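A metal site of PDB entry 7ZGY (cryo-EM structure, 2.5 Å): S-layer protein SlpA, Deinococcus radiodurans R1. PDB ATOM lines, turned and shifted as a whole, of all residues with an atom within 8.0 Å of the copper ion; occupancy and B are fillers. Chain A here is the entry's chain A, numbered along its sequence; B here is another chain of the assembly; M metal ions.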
ATOM      1  N   ARG A 519       8.395  10.184  21.540  1.00  0.00           N
ATOM      2  CA  ARG A 519       7.593  10.992  22.445  1.00  0.00           C
ATOM      3  C   ARG A 519       6.738  10.166  23.395  1.00  0.00           C
ATOM      4  O   ARG A 519       6.603  10.536  24.564  1.00  0.00           O
ATOM      5  CB  ARG A 519       6.691  11.951  21.661  1.00  0.00           C
ATOM      6  CG  ARG A 519       6.122  13.079  22.499  1.00  0.00           C
ATOM      7  CD  ARG A 519       5.731  14.267  21.633  1.00  0.00           C
ATOM      8  NE  ARG A 519       5.681  15.501  22.398  1.00  0.00           N
ATOM      9  CZ  ARG A 519       6.744  16.208  22.756  1.00  0.00           C
ATOM     10  NH1 ARG A 519       7.968  15.807  22.470  1.00  0.00           N
ATOM     11  NH2 ARG A 519       6.572  17.341  23.432  1.00  0.00           N
ATOM     12  N   GLY A 520       6.159   9.065  22.935  1.00  0.00           N
ATOM     13  CA  GLY A 520       5.287   8.295  23.800  1.00  0.00           C
ATOM     14  C   GLY A 520       4.750   7.072  23.089  1.00  0.00           C
ATOM     15  O   GLY A 520       5.281   6.643  22.061  1.00  0.00           O
ATOM     16  N   ASP A 521       3.676   6.533  23.658  1.00  0.00           N
ATOM     17  CA  ASP A 521       3.083   5.290  23.181  1.00  0.00           C
ATOM     18  C   ASP A 521       1.842   5.588  22.342  1.00  0.00           C
ATOM     19  O   ASP A 521       0.992   6.379  22.754  1.00  0.00           O
ATOM     20  CB  ASP A 521       2.713   4.379  24.355  1.00  0.00           C
ATOM     21  CG  ASP A 521       3.887   4.075  25.241  1.00  0.00           C
ATOM     22  OD1 ASP A 521       5.028   4.415  24.864  1.00  0.00           O
ATOM     23  OD2 ASP A 521       3.680   3.475  26.323  1.00  0.00           O
ATOM     24  N   GLY A 547      -0.576   9.742  20.016  1.00  0.00           N
ATOM     25  CA  GLY A 547       0.088   9.063  21.113  1.00  0.00           C
ATOM     26  C   GLY A 547      -0.138   9.753  22.438  1.00  0.00           C
ATOM     27  O   GLY A 547      -0.675  10.865  22.514  1.00  0.00           O
ATOM     28  N   SER A 548       0.289   9.060  23.489  1.00  0.00           N
ATOM     29  CA  SER A 548       0.312   9.568  24.856  1.00  0.00           C
ATOM     30  C   SER A 548       1.759   9.721  25.291  1.00  0.00           C
ATOM     31  O   SER A 548       2.541   8.774  25.188  1.00  0.00           O
ATOM     32  CB  SER A 548      -0.424   8.624  25.796  1.00  0.00           C
ATOM     33  OG  SER A 548      -0.287   9.023  27.146  1.00  0.00           O
ATOM     34  N   ARG A 549       2.111  10.914  25.781  1.00  0.00           N
ATOM     35  CA  ARG A 549       3.496  11.192  26.131  1.00  0.00           C
ATOM     36  C   ARG A 549       3.983  10.246  27.218  1.00  0.00           C
ATOM     37  O   ARG A 549       3.319  10.069  28.243  1.00  0.00           O
ATOM     38  CB  ARG A 549       3.633  12.642  26.605  1.00  0.00           C
ATOM     39  CG  ARG A 549       4.198  13.584  25.581  1.00  0.00           C
ATOM     40  CD  ARG A 549       4.454  14.956  26.174  1.00  0.00           C
ATOM     41  NE  ARG A 549       5.698  15.010  26.919  1.00  0.00           N
ATOM     42  CZ  ARG A 549       6.217  16.127  27.423  1.00  0.00           C
ATOM     43  NH1 ARG A 549       5.624  17.289  27.272  1.00  0.00           N
ATOM     44  NH2 ARG A 549       7.377  16.065  28.081  1.00  0.00           N
ATOM     45  N   SER A 550       5.150   9.660  26.998  1.00  0.00           N
ATOM     46  CA  SER A 550       5.794   8.782  27.959  1.00  0.00           C
ATOM     47  C   SER A 550       4.910   7.613  28.364  1.00  0.00           C
ATOM     48  O   SER A 550       5.154   6.972  29.391  1.00  0.00           O
ATOM     49  CB  SER A 550       6.243   9.555  29.202  1.00  0.00           C
ATOM     50  OG  SER A 550       7.070  10.641  28.846  1.00  0.00           O
ATOM     51  N   GLY A 551       3.884   7.307  27.584  1.00  0.00           N
ATOM     52  CA  GLY A 551       2.944   6.290  27.995  1.00  0.00           C
ATOM     53  C   GLY A 551       2.279   6.682  29.297  1.00  0.00           C
ATOM     54  O   GLY A 551       1.912   7.842  29.511  1.00  0.00           O
ATOM     55  N   LEU A 552       2.124   5.705  30.186  1.00  0.00           N
ATOM     56  CA  LEU A 552       1.570   5.972  31.506  1.00  0.00           C
ATOM     57  C   LEU A 552       2.712   6.224  32.485  1.00  0.00           C
ATOM     58  O   LEU A 552       3.638   5.421  32.598  1.00  0.00           O
ATOM     59  CB  LEU A 552       0.699   4.804  31.983  1.00  0.00           C
ATOM     60  CG  LEU A 552       1.367   3.454  32.225  1.00  0.00           C
ATOM     61  CD1 LEU A 552       1.858   3.350  33.653  1.00  0.00           C
ATOM     62  CD2 LEU A 552       0.383   2.344  31.917  1.00  0.00           C
ATOM     63  N   ASP A 553       2.635   7.350  33.197  1.00  0.00           N
ATOM     64  CA  ASP A 553       3.679   7.740  34.126  1.00  0.00           C
ATOM     65  C   ASP A 553       3.039   8.484  35.289  1.00  0.00           C
ATOM     66  O   ASP A 553       2.000   9.123  35.152  1.00  0.00           O
ATOM     67  CB  ASP A 553       4.736   8.607  33.429  1.00  0.00           C
ATOM     68  CG  ASP A 553       4.163   9.843  32.780  1.00  0.00           C
ATOM     69  OD1 ASP A 553       2.949  10.100  32.958  1.00  0.00           O
ATOM     70  OD2 ASP A 553       4.900  10.546  32.079  1.00  0.00           O
ATOM     71  N   GLY A 554       3.686   8.388  36.451  1.00  0.00           N
ATOM     72  CA  GLY A 554       3.135   8.946  37.656  1.00  0.00           C
ATOM     73  C   GLY A 554       3.046  10.458  37.619  1.00  0.00           C
ATOM     74  O   GLY A 554       3.744  11.141  36.879  1.00  0.00           O
ATOM     75  N   GLU A 557       5.112  14.144  36.635  1.00  0.00           N
ATOM     76  CA  GLU A 557       5.874  13.948  35.416  1.00  0.00           C
ATOM     77  C   GLU A 557       5.252  14.748  34.281  1.00  0.00           C
ATOM     78  O   GLU A 557       4.033  14.902  34.203  1.00  0.00           O
ATOM     79  CB  GLU A 557       5.926  12.463  35.040  1.00  0.00           C
ATOM     80  CG  GLU A 557       6.633  11.589  36.051  1.00  0.00           C
ATOM     81  CD  GLU A 557       7.037  10.242  35.495  1.00  0.00           C
ATOM     82  OE1 GLU A 557       7.575  10.211  34.367  1.00  0.00           O
ATOM     83  OE2 GLU A 557       6.820   9.223  36.168  1.00  0.00           O
ATOM     84  N   ALA A 558       6.120  15.267  33.410  1.00  0.00           N
ATOM     85  CA  ALA A 558       5.651  16.149  32.354  1.00  0.00           C
ATOM     86  C   ALA A 558       4.673  15.468  31.401  1.00  0.00           C
ATOM     87  O   ALA A 558       3.914  16.155  30.721  1.00  0.00           O
ATOM     88  CB  ALA A 558       6.840  16.701  31.559  1.00  0.00           C
ATOM     89  N   GLY A 559       4.687  14.140  31.338  1.00  0.00           N
ATOM     90  CA  GLY A 559       3.858  13.426  30.396  1.00  0.00           C
ATOM     91  C   GLY A 559       2.644  12.747  30.984  1.00  0.00           C
ATOM     92  O   GLY A 559       2.154  11.758  30.424  1.00  0.00           O
ATOM     93  N   TYR A 560       2.144  13.257  32.105  1.00  0.00           N
ATOM     94  CA  TYR A 560       0.966  12.683  32.748  1.00  0.00           C
ATOM     95  C   TYR A 560      -0.290  13.314  32.158  1.00  0.00           C
ATOM     96  O   TYR A 560      -0.461  14.529  32.209  1.00  0.00           O
ATOM     97  CB  TYR A 560       1.000  12.903  34.264  1.00  0.00           C
ATOM     98  CG  TYR A 560      -0.205  12.308  34.954  1.00  0.00           C
ATOM     99  CD1 TYR A 560      -0.255  10.962  35.290  1.00  0.00           C
ATOM    100  CD2 TYR A 560      -1.308  13.090  35.256  1.00  0.00           C
ATOM    101  CE1 TYR A 560      -1.345  10.413  35.912  1.00  0.00           C
ATOM    102  CE2 TYR A 560      -2.417  12.552  35.882  1.00  0.00           C
ATOM    103  CZ  TYR A 560      -2.428  11.217  36.201  1.00  0.00           C
ATOM    104  OH  TYR A 560      -3.528  10.676  36.829  1.00  0.00           O
ATOM    105  N   GLY A 561      -1.160  12.468  31.606  1.00  0.00           N
ATOM    106  CA  GLY A 561      -2.387  12.974  31.015  1.00  0.00           C
ATOM    107  C   GLY A 561      -2.162  13.929  29.873  1.00  0.00           C
ATOM    108  O   GLY A 561      -2.959  14.853  29.679  1.00  0.00           O
ATOM    109  N   VAL A 562      -1.089  13.742  29.114  1.00  0.00           N
ATOM    110  CA  VAL A 562      -0.754  14.610  27.989  1.00  0.00           C
ATOM    111  C   VAL A 562      -0.687  13.756  26.732  1.00  0.00           C
ATOM    112  O   VAL A 562      -0.003  12.725  26.711  1.00  0.00           O
ATOM    113  CB  VAL A 562       0.560  15.367  28.216  1.00  0.00           C
ATOM    114  CG1 VAL A 562       1.696  14.398  28.370  1.00  0.00           C
ATOM    115  CG2 VAL A 562       0.829  16.322  27.065  1.00  0.00           C
ATOM    116  N   TYR A 563      -1.408  14.176  25.702  1.00  0.00           N
ATOM    117  CA  TYR A 563      -1.520  13.421  24.462  1.00  0.00           C
ATOM    118  C   TYR A 563      -1.204  14.329  23.285  1.00  0.00           C
ATOM    119  O   TYR A 563      -1.509  15.529  23.300  1.00  0.00           O
ATOM    120  CB  TYR A 563      -2.917  12.814  24.298  1.00  0.00           C
ATOM    121  CG  TYR A 563      -3.292  11.873  25.420  1.00  0.00           C
ATOM    122  CD1 TYR A 563      -3.745  12.365  26.627  1.00  0.00           C
ATOM    123  CD2 TYR A 563      -3.169  10.508  25.270  1.00  0.00           C
ATOM    124  CE1 TYR A 563      -4.070  11.527  27.664  1.00  0.00           C
ATOM    125  CE2 TYR A 563      -3.497   9.656  26.303  1.00  0.00           C
ATOM    126  CZ  TYR A 563      -3.949  10.174  27.493  1.00  0.00           C
ATOM    127  OH  TYR A 563      -4.283   9.333  28.519  1.00  0.00           O
ATOM    128  N   ASN A 596      -1.595  17.152  37.676  1.00  0.00           N
ATOM    129  CA  ASN A 596      -0.380  16.918  36.900  1.00  0.00           C
ATOM    130  C   ASN A 596       0.812  17.713  37.391  1.00  0.00           C
ATOM    131  O   ASN A 596       1.945  17.252  37.230  1.00  0.00           O
ATOM    132  CB  ASN A 596      -0.606  17.236  35.415  1.00  0.00           C
ATOM    133  CG  ASN A 596       0.642  17.021  34.570  1.00  0.00           C
ATOM    134  OD1 ASN A 596       1.522  16.256  34.941  1.00  0.00           O
ATOM    135  ND2 ASN A 596       0.723  17.691  33.432  1.00  0.00           N
ATOM    136  N   TYR B 379      -9.252   6.672  35.745  1.00  0.00           N
ATOM    137  CA  TYR B 379      -8.422   7.031  34.605  1.00  0.00           C
ATOM    138  C   TYR B 379      -7.524   5.870  34.232  1.00  0.00           C
ATOM    139  O   TYR B 379      -6.945   5.215  35.104  1.00  0.00           O
ATOM    140  CB  TYR B 379      -7.572   8.268  34.904  1.00  0.00           C
ATOM    141  CG  TYR B 379      -6.846   8.827  33.711  1.00  0.00           C
ATOM    142  CD1 TYR B 379      -7.457   8.893  32.463  1.00  0.00           C
ATOM    143  CD2 TYR B 379      -5.540   9.294  33.826  1.00  0.00           C
ATOM    144  CE1 TYR B 379      -6.791   9.401  31.369  1.00  0.00           C
ATOM    145  CE2 TYR B 379      -4.870   9.810  32.727  1.00  0.00           C
ATOM    146  CZ  TYR B 379      -5.507   9.858  31.513  1.00  0.00           C
ATOM    147  OH  TYR B 379      -4.850  10.368  30.417  1.00  0.00           O
ATOM    148  N   GLU B 381      -4.384   5.955  31.918  1.00  0.00           N
ATOM    149  CA  GLU B 381      -3.509   6.768  31.085  1.00  0.00           C
ATOM    150  C   GLU B 381      -3.090   5.982  29.861  1.00  0.00           C
ATOM    151  O   GLU B 381      -2.668   4.821  29.973  1.00  0.00           O
ATOM    152  CB  GLU B 381      -2.282   7.231  31.876  1.00  0.00           C
ATOM    153  CG  GLU B 381      -1.668   8.498  31.338  1.00  0.00           C
ATOM    154  CD  GLU B 381      -0.304   8.769  31.930  1.00  0.00           C
ATOM    155  OE1 GLU B 381      -0.071   8.358  33.082  1.00  0.00           O
ATOM    156  OE2 GLU B 381       0.527   9.403  31.244  1.00  0.00           O
ATOM    157  N   GLY B 382      -3.200   6.594  28.697  1.00  0.00           N
ATOM    158  CA  GLY B 382      -2.933   5.902  27.460  1.00  0.00           C
ATOM    159  C   GLY B 382      -1.537   5.324  27.395  1.00  0.00           C
ATOM    160  O   GLY B 382      -0.555   6.033  27.615  1.00  0.00           O
ATOM    161  N   SER B 383      -1.445   4.025  27.106  1.00  0.00           N
ATOM    162  CA  SER B 383      -0.145   3.389  26.940  1.00  0.00           C
ATOM    163  C   SER B 383      -0.301   2.174  26.040  1.00  0.00           C
ATOM    164  O   SER B 383      -1.388   1.618  25.892  1.00  0.00           O
ATOM    165  CB  SER B 383       0.450   2.970  28.293  1.00  0.00           C
ATOM    166  OG  SER B 383      -0.218   1.839  28.810  1.00  0.00           O
HETATM  167 CU    CU M   1       1.686  10.109  29.943  1.00  0.00          CU
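The side-chain carboxylate of Glu 381 of chain B lies within hydrogen-bond range of the backbone NH of Asp 553 (2.9 Å).
The backbone carbonyl oxygen of Gly 551 lies close to the side-chain hydroxyl of Ser 548 (3.4 Å).
The backbone NH (N) of Arg 549 is in hydrogen-bond range of the backbone carbonyl oxygen (O) of Val 562 (2.9 Å).
The backbone NH (N) of Tyr 560 lies close to the side-chain carboxylate (OD1) of Asp 553.
The side-chain hydroxyl (OG) of Ser 548 sits at hydrogen-bond distance from the backbone carbonyl oxygen (O) of Gly 382 of chain B (3.0 Å).
O of Asp 521 is in hydrogen-bond range of N of Ser 548, 2.9 Å away.
Ser 548 touches the copper ion.
Asp 553 touches the copper ion (OD1 to CU, 3.3 Å).
Tyr 560 touches the copper ion.
Seven residues have an atom within 4 Å of the copper ion: Ser 548, Arg 549, Gly 551, Asp 553, Gly 559, Tyr 560 and Glu 381 of chain B.
Along chain A the residues within 4 Å of the copper ion span positions 548 to 560.
The copper ion is bound by O of Gly 559 (1.8 Å), OE2 of Glu 381 of chain B (1.9 Å), O of Gly 551 (2.3 Å) and O of Arg 549 (2.4 Å).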
